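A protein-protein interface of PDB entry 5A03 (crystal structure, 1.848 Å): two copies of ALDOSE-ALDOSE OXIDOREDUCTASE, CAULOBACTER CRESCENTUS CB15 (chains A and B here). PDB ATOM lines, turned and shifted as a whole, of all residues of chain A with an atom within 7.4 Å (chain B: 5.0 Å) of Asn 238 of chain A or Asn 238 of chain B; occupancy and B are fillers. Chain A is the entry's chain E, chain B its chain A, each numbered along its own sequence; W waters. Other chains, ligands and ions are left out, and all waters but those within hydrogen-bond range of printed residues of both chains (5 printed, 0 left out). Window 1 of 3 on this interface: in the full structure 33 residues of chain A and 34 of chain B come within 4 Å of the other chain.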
ATOM      1  N   THR A 156      32.155  25.445 -27.709  1.00  0.00           N
ATOM      2  CA  THR A 156      30.725  25.487 -27.397  1.00  0.00           C
ATOM      3  C   THR A 156      30.285  24.280 -26.601  1.00  0.00           C
ATOM      4  O   THR A 156      30.772  23.172 -26.830  1.00  0.00           O
ATOM      5  CB  THR A 156      29.825  25.545 -28.657  1.00  0.00           C
ATOM      6  OG1 THR A 156      29.963  24.341 -29.423  1.00  0.00           O
ATOM      7  CG2 THR A 156      30.152  26.762 -29.531  1.00  0.00           C
ATOM      8  N   VAL A 157      29.344  24.517 -25.684  1.00  0.00           N
ATOM      9  CA  VAL A 157      28.576  23.463 -25.029  1.00  0.00           C
ATOM     10  C   VAL A 157      27.120  23.823 -25.231  1.00  0.00           C
ATOM     11  O   VAL A 157      26.684  24.915 -24.878  1.00  0.00           O
ATOM     12  CB  VAL A 157      28.871  23.334 -23.518  1.00  0.00           C
ATOM     13  CG1 VAL A 157      27.903  22.326 -22.865  1.00  0.00           C
ATOM     14  CG2 VAL A 157      30.316  22.920 -23.283  1.00  0.00           C
ATOM     15  N   VAL A 158      26.384  22.921 -25.852  1.00  0.00           N
ATOM     16  CA  VAL A 158      24.975  23.121 -26.089  1.00  0.00           C
ATOM     17  C   VAL A 158      24.266  22.009 -25.359  1.00  0.00           C
ATOM     18  O   VAL A 158      24.449  20.846 -25.670  1.00  0.00           O
ATOM     19  CB  VAL A 158      24.618  23.102 -27.595  1.00  0.00           C
ATOM     20  CG1 VAL A 158      23.090  23.196 -27.793  1.00  0.00           C
ATOM     21  CG2 VAL A 158      25.332  24.233 -28.319  1.00  0.00           C
ATOM     22  N   THR A 159      23.461  22.374 -24.369  1.00  0.00           N
ATOM     23  CA  THR A 159      22.895  21.370 -23.484  1.00  0.00           C
ATOM     24  C   THR A 159      21.466  21.740 -23.086  1.00  0.00           C
ATOM     25  O   THR A 159      21.191  22.880 -22.701  1.00  0.00           O
ATOM     26  CB  THR A 159      23.793  21.185 -22.238  1.00  0.00           C
ATOM     27  OG1 THR A 159      23.221  20.207 -21.356  1.00  0.00           O
ATOM     28  CG2 THR A 159      24.006  22.515 -21.502  1.00  0.00           C
ATOM     29  N   ASP A 160      20.566  20.763 -23.194  1.00  0.00           N
ATOM     30  CA  ASP A 160      19.146  20.953 -22.916  1.00  0.00           C
ATOM     31  C   ASP A 160      18.663  19.941 -21.879  1.00  0.00           C
ATOM     32  O   ASP A 160      18.808  18.739 -22.072  1.00  0.00           O
ATOM     33  CB  ASP A 160      18.311  20.794 -24.194  1.00  0.00           C
ATOM     34  CG  ASP A 160      18.853  21.622 -25.366  1.00  0.00           C
ATOM     35  OD1 ASP A 160      19.430  22.707 -25.112  1.00  0.00           O
ATOM     36  OD2 ASP A 160      18.696  21.189 -26.538  1.00  0.00           O
ATOM     37  N   SER A 190      22.093  21.140 -16.918  1.00  0.00           N
ATOM     38  CA  SER A 190      22.705  21.852 -18.033  1.00  0.00           C
ATOM     39  C   SER A 190      23.875  22.669 -17.521  1.00  0.00           C
ATOM     40  O   SER A 190      24.964  22.655 -18.091  1.00  0.00           O
ATOM     41  CB  SER A 190      21.690  22.764 -18.726  1.00  0.00           C
ATOM     42  OG  SER A 190      20.660  22.021 -19.349  1.00  0.00           O
ATOM     43  N   ALA A 194      27.844  22.136 -18.229  1.00  0.00           N
ATOM     44  CA  ALA A 194      28.670  23.179 -18.854  1.00  0.00           C
ATOM     45  C   ALA A 194      29.949  23.418 -18.042  1.00  0.00           C
ATOM     46  O   ALA A 194      31.044  23.574 -18.605  1.00  0.00           O
ATOM     47  CB  ALA A 194      27.879  24.479 -19.017  1.00  0.00           C
ATOM     48  N   VAL A 208      16.875  34.199 -20.607  1.00  0.00           N
ATOM     49  CA  VAL A 208      15.539  34.494 -21.081  1.00  0.00           C
ATOM     50  C   VAL A 208      14.555  33.544 -20.414  1.00  0.00           C
ATOM     51  O   VAL A 208      14.762  32.330 -20.448  1.00  0.00           O
ATOM     52  CB  VAL A 208      15.436  34.318 -22.612  1.00  0.00           C
ATOM     53  CG1 VAL A 208      13.981  34.311 -23.051  1.00  0.00           C
ATOM     54  CG2 VAL A 208      16.221  35.413 -23.330  1.00  0.00           C
ATOM     55  N   ILE A 225      13.564  28.592 -18.608  1.00  0.00           N
ATOM     56  CA  ILE A 225      14.531  29.660 -18.480  1.00  0.00           C
ATOM     57  C   ILE A 225      15.812  29.196 -19.153  1.00  0.00           C
ATOM     58  O   ILE A 225      16.481  28.250 -18.701  1.00  0.00           O
ATOM     59  CB  ILE A 225      14.762  30.087 -17.004  1.00  0.00           C
ATOM     60  CG1 ILE A 225      15.842  31.179 -16.931  1.00  0.00           C
ATOM     61  CG2 ILE A 225      15.077  28.874 -16.100  1.00  0.00           C
ATOM     62  CD1 ILE A 225      15.813  32.001 -15.623  1.00  0.00           C
ATOM     63  N   ASN A 226      16.105  29.817 -20.296  1.00  0.00           N
ATOM     64  CA  ASN A 226      17.292  29.450 -21.055  1.00  0.00           C
ATOM     65  C   ASN A 226      18.429  30.420 -20.771  1.00  0.00           C
ATOM     66  O   ASN A 226      18.200  31.603 -20.523  1.00  0.00           O
ATOM     67  CB  ASN A 226      16.981  29.400 -22.558  1.00  0.00           C
ATOM     68  CG  ASN A 226      15.856  28.422 -22.887  1.00  0.00           C
ATOM     69  OD1 ASN A 226      15.608  27.477 -22.138  1.00  0.00           O
ATOM     70  ND2 ASN A 226      15.166  28.653 -23.998  1.00  0.00           N
ATOM     71  N   PHE A 227      19.665  29.935 -20.795  1.00  0.00           N
ATOM     72  CA  PHE A 227      20.739  30.831 -20.421  1.00  0.00           C
ATOM     73  C   PHE A 227      21.987  30.596 -21.242  1.00  0.00           C
ATOM     74  O   PHE A 227      22.186  29.517 -21.822  1.00  0.00           O
ATOM     75  CB  PHE A 227      21.045  30.717 -18.912  1.00  0.00           C
ATOM     76  CG  PHE A 227      21.220  29.300 -18.403  1.00  0.00           C
ATOM     77  CD1 PHE A 227      20.118  28.518 -18.094  1.00  0.00           C
ATOM     78  CD2 PHE A 227      22.490  28.778 -18.180  1.00  0.00           C
ATOM     79  CE1 PHE A 227      20.273  27.227 -17.600  1.00  0.00           C
ATOM     80  CE2 PHE A 227      22.655  27.483 -17.679  1.00  0.00           C
ATOM     81  CZ  PHE A 227      21.545  26.710 -17.387  1.00  0.00           C
ATOM     82  N   GLN A 228      22.801  31.641 -21.314  1.00  0.00           N
ATOM     83  CA  GLN A 228      24.097  31.598 -21.981  1.00  0.00           C
ATOM     84  C   GLN A 228      25.208  31.807 -20.988  1.00  0.00           C
ATOM     85  O   GLN A 228      25.082  32.634 -20.091  1.00  0.00           O
ATOM     86  CB  GLN A 228      24.195  32.689 -23.043  1.00  0.00           C
ATOM     87  CG  GLN A 228      23.101  32.662 -24.040  1.00  0.00           C
ATOM     88  CD  GLN A 228      23.362  33.642 -25.136  1.00  0.00           C
ATOM     89  OE1 GLN A 228      23.321  34.854 -24.912  1.00  0.00           O
ATOM     90  NE2 GLN A 228      23.668  33.134 -26.331  1.00  0.00           N
ATOM     91  N   LEU A 229      26.310  31.089 -21.175  1.00  0.00           N
ATOM     92  CA  LEU A 229      27.459  31.243 -20.301  1.00  0.00           C
ATOM     93  C   LEU A 229      28.677  31.547 -21.139  1.00  0.00           C
ATOM     94  O   LEU A 229      28.857  30.970 -22.221  1.00  0.00           O
ATOM     95  CB  LEU A 229      27.706  29.974 -19.464  1.00  0.00           C
ATOM     96  CG  LEU A 229      26.528  29.446 -18.635  1.00  0.00           C
ATOM     97  CD1 LEU A 229      26.859  28.079 -18.037  1.00  0.00           C
ATOM     98  CD2 LEU A 229      26.166  30.452 -17.535  1.00  0.00           C
ATOM     99  N   PHE A 231      32.903  31.613 -20.559  1.00  0.00           N
ATOM    100  CA  PHE A 231      33.958  31.180 -19.646  1.00  0.00           C
ATOM    101  C   PHE A 231      35.250  31.918 -19.972  1.00  0.00           C
ATOM    102  O   PHE A 231      35.391  32.431 -21.082  1.00  0.00           O
ATOM    103  CB  PHE A 231      34.171  29.663 -19.746  1.00  0.00           C
ATOM    104  CG  PHE A 231      32.978  28.861 -19.316  1.00  0.00           C
ATOM    105  CD1 PHE A 231      32.824  28.490 -17.997  1.00  0.00           C
ATOM    106  CD2 PHE A 231      32.017  28.472 -20.240  1.00  0.00           C
ATOM    107  CE1 PHE A 231      31.729  27.751 -17.593  1.00  0.00           C
ATOM    108  CE2 PHE A 231      30.914  27.721 -19.846  1.00  0.00           C
ATOM    109  CZ  PHE A 231      30.770  27.365 -18.520  1.00  0.00           C
ATOM    110  N   THR A 236      31.992  28.846 -24.624  1.00  0.00           N
ATOM    111  CA  THR A 236      30.634  29.351 -24.464  1.00  0.00           C
ATOM    112  C   THR A 236      29.683  28.213 -24.208  1.00  0.00           C
ATOM    113  O   THR A 236      29.948  27.078 -24.608  1.00  0.00           O
ATOM    114  CB  THR A 236      30.153  30.114 -25.723  1.00  0.00           C
ATOM    115  OG1 THR A 236      30.111  29.205 -26.838  1.00  0.00           O
ATOM    116  CG2 THR A 236      31.091  31.286 -26.046  1.00  0.00           C
ATOM    117  N   ALA A 237      28.560  28.508 -23.564  1.00  0.00           N
ATOM    118  CA  ALA A 237      27.484  27.524 -23.445  1.00  0.00           C
ATOM    119  C   ALA A 237      26.120  28.124 -23.714  1.00  0.00           C
ATOM    120  O   ALA A 237      25.838  29.244 -23.289  1.00  0.00           O
ATOM    121  CB  ALA A 237      27.496  26.878 -22.049  1.00  0.00           C
ATOM    122  N   ASN A 238      25.293  27.366 -24.434  1.00  0.00           N
ATOM    123  CA  ASN A 238      23.881  27.644 -24.632  1.00  0.00           C
ATOM    124  C   ASN A 238      23.125  26.555 -23.916  1.00  0.00           C
ATOM    125  O   ASN A 238      23.293  25.378 -24.258  1.00  0.00           O
ATOM    126  CB  ASN A 238      23.479  27.617 -26.114  1.00  0.00           C
ATOM    127  CG  ASN A 238      23.522  28.986 -26.791  1.00  0.00           C
ATOM    128  OD1 ASN A 238      23.905  30.002 -26.205  1.00  0.00           O
ATOM    129  ND2 ASN A 238      23.117  29.006 -28.063  1.00  0.00           N
ATOM    130  N   CYS A 239      22.269  26.930 -22.969  1.00  0.00           N
ATOM    131  CA  CYS A 239      21.576  25.942 -22.139  1.00  0.00           C
ATOM    132  C   CYS A 239      20.058  26.126 -22.098  1.00  0.00           C
ATOM    133  O   CYS A 239      19.571  27.255 -21.980  1.00  0.00           O
ATOM    134  CB  CYS A 239      22.117  26.002 -20.706  1.00  0.00           C
ATOM    135  SG  CYS A 239      23.906  25.996 -20.585  1.00  0.00           S
ATOM    136  N   VAL A 240      19.322  25.016 -22.174  1.00  0.00           N
ATOM    137  CA  VAL A 240      17.872  25.030 -21.961  1.00  0.00           C
ATOM    138  C   VAL A 240      17.555  24.430 -20.592  1.00  0.00           C
ATOM    139  O   VAL A 240      18.185  23.462 -20.172  1.00  0.00           O
ATOM    140  CB  VAL A 240      17.098  24.244 -23.060  1.00  0.00           C
ATOM    141  CG1 VAL A 240      15.662  23.983 -22.647  1.00  0.00           C
ATOM    142  CG2 VAL A 240      17.115  25.023 -24.397  1.00  0.00           C
ATOM    143  N   SER A 241      16.599  25.047 -19.907  1.00  0.00           N
ATOM    144  CA  SER A 241      15.970  24.502 -18.704  1.00  0.00           C
ATOM    145  C   SER A 241      14.471  24.598 -18.909  1.00  0.00           C
ATOM    146  O   SER A 241      13.989  25.676 -19.226  1.00  0.00           O
ATOM    147  CB  SER A 241      16.364  25.300 -17.459  1.00  0.00           C
ATOM    148  OG  SER A 241      15.680  24.796 -16.320  1.00  0.00           O
ATOM    149  N   ARG A 249      20.304  16.256 -22.854  1.00  0.00           N
ATOM    150  CA  ARG A 249      21.419  16.072 -23.764  1.00  0.00           C
ATOM    151  C   ARG A 249      22.459  17.147 -23.611  1.00  0.00           C
ATOM    152  O   ARG A 249      22.183  18.227 -23.084  1.00  0.00           O
ATOM    153  CB  ARG A 249      20.923  16.063 -25.220  1.00  0.00           C
ATOM    154  CG  ARG A 249      20.311  17.407 -25.649  1.00  0.00           C
ATOM    155  CD  ARG A 249      19.742  17.356 -27.058  1.00  0.00           C
ATOM    156  NE  ARG A 249      19.417  18.691 -27.544  1.00  0.00           N
ATOM    157  CZ  ARG A 249      19.459  19.045 -28.822  1.00  0.00           C
ATOM    158  NH1 ARG A 249      19.787  18.148 -29.743  1.00  0.00           N
ATOM    159  NH2 ARG A 249      19.150  20.288 -29.176  1.00  0.00           N
ATOM    160  N   ARG A 251      26.029  18.529 -26.217  1.00  0.00           N
ATOM    161  CA  ARG A 251      27.141  18.364 -27.138  1.00  0.00           C
ATOM    162  C   ARG A 251      28.237  19.334 -26.762  1.00  0.00           C
ATOM    163  O   ARG A 251      27.978  20.522 -26.580  1.00  0.00           O
ATOM    164  CB  ARG A 251      26.726  18.617 -28.587  1.00  0.00           C
ATOM    165  CG  ARG A 251      27.903  18.466 -29.549  1.00  0.00           C
ATOM    166  CD  ARG A 251      27.512  18.817 -30.990  1.00  0.00           C
ATOM    167  NE  ARG A 251      26.508  17.897 -31.531  1.00  0.00           N
ATOM    168  CZ  ARG A 251      26.079  17.943 -32.791  1.00  0.00           C
ATOM    169  NH1 ARG A 251      26.576  18.860 -33.615  1.00  0.00           N
ATOM    170  NH2 ARG A 251      25.154  17.088 -33.228  1.00  0.00           N
ATOM    171  N   VAL B 157      13.459  26.202 -29.686  1.00  0.00           N
ATOM    172  CA  VAL B 157      14.228  25.855 -30.873  1.00  0.00           C
ATOM    173  C   VAL B 157      15.693  25.942 -30.484  1.00  0.00           C
ATOM    174  O   VAL B 157      16.154  26.997 -30.048  1.00  0.00           O
ATOM    175  CB  VAL B 157      13.950  26.805 -32.052  1.00  0.00           C
ATOM    176  CG1 VAL B 157      14.908  26.491 -33.229  1.00  0.00           C
ATOM    177  CG2 VAL B 157      12.492  26.720 -32.472  1.00  0.00           C
ATOM    178  N   VAL B 158      16.416  24.836 -30.606  1.00  0.00           N
ATOM    179  CA  VAL B 158      17.845  24.832 -30.328  1.00  0.00           C
ATOM    180  C   VAL B 158      18.571  24.521 -31.628  1.00  0.00           C
ATOM    181  O   VAL B 158      18.420  23.431 -32.183  1.00  0.00           O
ATOM    182  CB  VAL B 158      18.221  23.797 -29.240  1.00  0.00           C
ATOM    183  CG1 VAL B 158      19.730  23.749 -29.043  1.00  0.00           C
ATOM    184  CG2 VAL B 158      17.509  24.125 -27.934  1.00  0.00           C
ATOM    185  N   THR B 159      19.340  25.483 -32.124  1.00  0.00           N
ATOM    186  CA  THR B 159      19.896  25.342 -33.455  1.00  0.00           C
ATOM    187  C   THR B 159      21.327  25.878 -33.503  1.00  0.00           C
ATOM    188  O   THR B 159      21.628  26.974 -33.006  1.00  0.00           O
ATOM    189  CB  THR B 159      18.991  26.048 -34.509  1.00  0.00           C
ATOM    190  OG1 THR B 159      19.562  25.909 -35.820  1.00  0.00           O
ATOM    191  CG2 THR B 159      18.800  27.541 -34.183  1.00  0.00           C
ATOM    192  N   ASP B 160      22.207  25.068 -34.086  1.00  0.00           N
ATOM    193  CA  ASP B 160      23.634  25.336 -34.124  1.00  0.00           C
ATOM    194  C   ASP B 160      24.130  25.312 -35.556  1.00  0.00           C
ATOM    195  O   ASP B 160      23.957  24.303 -36.240  1.00  0.00           O
ATOM    196  CB  ASP B 160      24.417  24.277 -33.332  1.00  0.00           C
ATOM    197  CG  ASP B 160      23.935  24.120 -31.911  1.00  0.00           C
ATOM    198  OD1 ASP B 160      23.390  25.091 -31.345  1.00  0.00           O
ATOM    199  OD2 ASP B 160      24.114  23.007 -31.354  1.00  0.00           O
ATOM    200  N   ASN B 226      26.786  33.538 -30.179  1.00  0.00           N
ATOM    201  CA  ASN B 226      25.582  32.796 -29.858  1.00  0.00           C
ATOM    202  C   ASN B 226      24.497  33.731 -29.387  1.00  0.00           C
ATOM    203  O   ASN B 226      24.781  34.735 -28.743  1.00  0.00           O
ATOM    204  CB  ASN B 226      25.882  31.744 -28.783  1.00  0.00           C
ATOM    205  CG  ASN B 226      27.024  30.822 -29.182  1.00  0.00           C
ATOM    206  OD1 ASN B 226      27.272  30.607 -30.372  1.00  0.00           O
ATOM    207  ND2 ASN B 226      27.730  30.281 -28.192  1.00  0.00           N
ATOM    208  N   PHE B 227      23.249  33.407 -29.691  1.00  0.00           N
ATOM    209  CA  PHE B 227      22.184  34.303 -29.318  1.00  0.00           C
ATOM    210  C   PHE B 227      20.933  33.579 -28.885  1.00  0.00           C
ATOM    211  O   PHE B 227      20.713  32.410 -29.212  1.00  0.00           O
ATOM    212  CB  PHE B 227      21.867  35.266 -30.470  1.00  0.00           C
ATOM    213  CG  PHE B 227      21.682  34.590 -31.809  1.00  0.00           C
ATOM    214  CD1 PHE B 227      22.784  34.197 -32.563  1.00  0.00           C
ATOM    215  CD2 PHE B 227      20.410  34.365 -32.316  1.00  0.00           C
ATOM    216  CE1 PHE B 227      22.615  33.590 -33.827  1.00  0.00           C
ATOM    217  CE2 PHE B 227      20.234  33.773 -33.577  1.00  0.00           C
ATOM    218  CZ  PHE B 227      21.344  33.377 -34.318  1.00  0.00           C
ATOM    219  N   GLN B 228      20.122  34.306 -28.129  1.00  0.00           N
ATOM    220  CA  GLN B 228      18.811  33.849 -27.676  1.00  0.00           C
ATOM    221  C   GLN B 228      17.742  34.725 -28.287  1.00  0.00           C
ATOM    222  O   GLN B 228      17.917  35.948 -28.373  1.00  0.00           O
ATOM    223  CB  GLN B 228      18.703  33.923 -26.161  1.00  0.00           C
ATOM    224  CG  GLN B 228      19.798  33.167 -25.439  1.00  0.00           C
ATOM    225  CD  GLN B 228      19.584  33.184 -23.941  1.00  0.00           C
ATOM    226  OE1 GLN B 228      19.679  34.236 -23.298  1.00  0.00           O
ATOM    227  NE2 GLN B 228      19.268  32.021 -23.374  1.00  0.00           N
ATOM    228  N   THR B 236      10.931  30.188 -27.509  1.00  0.00           N
ATOM    229  CA  THR B 236      12.304  30.633 -27.290  1.00  0.00           C
ATOM    230  C   THR B 236      13.257  29.940 -28.258  1.00  0.00           C
ATOM    231  O   THR B 236      12.988  28.823 -28.707  1.00  0.00           O
ATOM    232  CB  THR B 236      12.760  30.342 -25.842  1.00  0.00           C
ATOM    233  OG1 THR B 236      12.786  28.925 -25.628  1.00  0.00           O
ATOM    234  CG2 THR B 236      11.788  30.961 -24.837  1.00  0.00           C
ATOM    235  N   ALA B 237      14.377  30.588 -28.565  1.00  0.00           N
ATOM    236  CA  ALA B 237      15.437  29.939 -29.323  1.00  0.00           C
ATOM    237  C   ALA B 237      16.793  30.198 -28.702  1.00  0.00           C
ATOM    238  O   ALA B 237      17.093  31.325 -28.284  1.00  0.00           O
ATOM    239  CB  ALA B 237      15.437  30.409 -30.783  1.00  0.00           C
ATOM    240  N   ASN B 238      17.599  29.138 -28.651  1.00  0.00           N
ATOM    241  CA  ASN B 238      19.030  29.189 -28.354  1.00  0.00           C
ATOM    242  C   ASN B 238      19.787  28.866 -29.634  1.00  0.00           C
ATOM    243  O   ASN B 238      19.631  27.772 -30.185  1.00  0.00           O
ATOM    244  CB  ASN B 238      19.420  28.167 -27.272  1.00  0.00           C
ATOM    245  CG  ASN B 238      19.310  28.711 -25.858  1.00  0.00           C
ATOM    246  OD1 ASN B 238      18.882  29.849 -25.631  1.00  0.00           O
ATOM    247  ND2 ASN B 238      19.666  27.875 -24.890  1.00  0.00           N
ATOM    248  N   CYS B 239      20.615  29.795 -30.099  1.00  0.00           N
ATOM    249  CA  CYS B 239      21.280  29.641 -31.379  1.00  0.00           C
ATOM    250  C   CYS B 239      22.775  29.801 -31.252  1.00  0.00           C
ATOM    251  O   CYS B 239      23.258  30.719 -30.562  1.00  0.00           O
ATOM    252  CB  CYS B 239      20.735  30.669 -32.378  1.00  0.00           C
ATOM    253  SG  CYS B 239      18.934  30.759 -32.485  1.00  0.00           S
ATOM    254  N   VAL B 240      23.509  28.926 -31.935  1.00  0.00           N
ATOM    255  CA  VAL B 240      24.964  29.057 -32.065  1.00  0.00           C
ATOM    256  C   VAL B 240      25.326  29.503 -33.469  1.00  0.00           C
ATOM    257  O   VAL B 240      24.735  29.032 -34.449  1.00  0.00           O
ATOM    258  CB  VAL B 240      25.694  27.732 -31.755  1.00  0.00           C
ATOM    259  CG1 VAL B 240      27.125  27.719 -32.323  1.00  0.00           C
ATOM    260  CG2 VAL B 240      25.709  27.476 -30.251  1.00  0.00           C
HETATM  261  O   HOH W   1      16.372  30.986 -25.473  1.00  0.00           O
HETATM  262  O   HOH W   2      19.925  21.017 -31.881  1.00  0.00           O
HETATM  263  O   HOH W   3      22.191  26.669 -29.342  1.00  0.00           O
HETATM  264  O   HOH W   4      20.549  25.096 -25.542  1.00  0.00           O
HETATM  265  O   HOH W   5      26.477  30.992 -25.478  1.00  0.00           O
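Among the printed residues, pairs that only touch across the chains: Asp 160 of chain A with Val 158 of chain B (3.5 Å), Val 158 of chain A with Asp 160 of chain B (3.5 Å), Arg 249 of chain A with Val 158 of chain B (3.5 Å), Gln 228 of chain A with Gln 228 of chain B (3.6 Å), Val 158 of chain A with Val 158 of chain B (3.6 Å), Asn 226 of chain A with Asn 238 of chain B (3.6 Å), Val 208 of chain A with Gln 228 of chain B (3.7 Å), Val 240 of chain A with Val 158 of chain B (3.7 Å), Asn 238 of chain A with Asn 238 of chain B (3.7 Å), Asn 238 of chain A with Asn 226 of chain B (3.7 Å), Asn 238 of chain A with Val 240 of chain B (3.7 Å), Val 158 of chain A with Val 240 of chain B (3.8 Å) and Val 240 of chain A with Asn 238 of chain B (3.9 Å).
O of Asn 226 of chain B lies within hydrogen-bond range of NE2 of Gln 228 of chain A.
ND2 of Asn 226 of chain B sits at hydrogen-bond distance from OG1 of Thr 236 of chain A (2.9 Å).
N of Phe 227 of chain B sits close to NE2 of Gln 228 of chain A (3.4 Å).
NE2 of Gln 228 of chain B is in hydrogen-bond range of O of Asn 226 of chain A, at 3.1 Å.
The side-chain amide nitrogen of Gln 228 of chain B lies close to the backbone NH of Phe 227 of chain A (3.3 Å).
The side-chain amide nitrogen (ND2) of Asn 226 of chain A lies within hydrogen-bond range of the side-chain hydroxyl (OG1) of Thr 236 of chain B.
O of Cys 239 of chain A sits at hydrogen-bond distance from ND2 of Asn 238 of chain B (3.0 Å).
The side-chain amide nitrogen (ND2) of Asn 238 of chain A sits at hydrogen-bond distance from the backbone carbonyl oxygen (O) of Cys 239 of chain B, 3.0 Å away.
Asn 226 of chain A touches Gln 228 of chain B, and with the chains exchanged Gln 228 of chain A touches Asn 226 of chain B.
Asn 226 of chain A touches Asn 238 of chain B, and with the chains exchanged Asn 238 of chain A touches Asn 226 of chain B.
Gln 228 of chain B touches its own counterpart, Gln 228 of chain A.
Asn 238 of chain A touches Cys 239 of chain B, and with the chains exchanged Cys 239 of chain A touches Asn 238 of chain B.
Positions printed for both chains: 157, 158, 159, 160, 226, 227, 228, 236, 237, 238, 239 and 240.
Of the 21 pairs that touch across the chains among the printed residues, 19 have their exchanged pair printed and touching as well.
Asn 238 of chain A touches just these residues of chain B: Asn 226 (3.7 Å), Asn 238 (3.7 Å), Cys 239 (3.0 Å) and Val 240 (3.7 Å).
Asn 238 of chain B touches four residues of chain A.
Of the printed residues of chain A, Val 158 of chain B touches Val 158, Asp 160, Val 240 and Arg 249.
Printed residues of chain B within 4 Å of Cys 239 of chain A: Asn 238 (3.0 Å).
Of the printed residues of chain A, Cys 239 of chain B touches Asn 238 (3.0 Å).
Printed residues of chain B within 4 Å of Arg 249 of chain A: Val 158.
Printed residues of chain A within 4 Å of Gln 228 of chain B: Val 208, Asn 226, Phe 227 and Gln 228.
The nearest residue of chain B that does not touch Asn 238 of chain A is Phe 227 of chain B (4.3 Å).
The nearest residue of chain A that does not touch Asn 238 of chain B is Phe 227 of chain A (4.3 Å).
Of the 22 printed residues of chain A, 11 touch a printed residue of chain B.
Among the printed residues, 21 pairs touch across the chains.
Water W4 lies within hydrogen-bond range of the side-chain carboxylate of Asp 160 of chain A (2.7 Å), the side-chain amide nitrogen of Asn 238 of chain B (3.0 Å) and the backbone carbonyl oxygen of Asn 238 of chain A (3.0 Å).
Water W1 lies within hydrogen-bond range of the side-chain amide oxygen of Asn 238 of chain B (2.8 Å), the backbone carbonyl oxygen of Ala 237 of chain B (2.9 Å) and the side-chain amide nitrogen of Asn 226 of chain A (3.0 Å).
Water W3 lies within hydrogen-bond range of the side-chain carboxylate of Asp 160 of chain B (2.8 Å), the side-chain amide nitrogen of Asn 238 of chain A (2.8 Å) and the backbone carbonyl oxygen of Asn 238 of chain B (2.9 Å).
Water W5 lies within hydrogen-bond range of the side-chain amide oxygen (OD1) of Asn 238 of chain A, the backbone carbonyl oxygen (O) of Ala 237 of chain A and the side-chain amide nitrogen (ND2) of Asn 226 of chain B.
Water W2 lies within hydrogen-bond range of the backbone carbonyl oxygen of Val 158 of chain B (2.9 Å) and the guanidinium group of Arg 249 of chain A (2.9 Å).
O of Phe 227 of chain B sits at hydrogen-bond distance from N of Cys 239 of chain B (2.8 Å).
O of Val 158 of chain A is in hydrogen-bond range of N of Arg 251 of chain A, at 2.9 Å.
N of Thr 159 of chain A sits at hydrogen-bond distance from O of Asn 238 of chain A (3.0 Å).
The backbone NH (N) of Val 240 of chain A sits at hydrogen-bond distance from the backbone carbonyl oxygen (O) of Thr 159 of chain A (2.9 Å).
The backbone carbonyl oxygen of Val 208 of chain A lies within hydrogen-bond range of the backbone NH of Asn 226 of chain A (2.9 Å).
The backbone carbonyl oxygen (O) of Phe 227 of chain A lies within hydrogen-bond range of the backbone NH (N) of Cys 239 of chain A.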
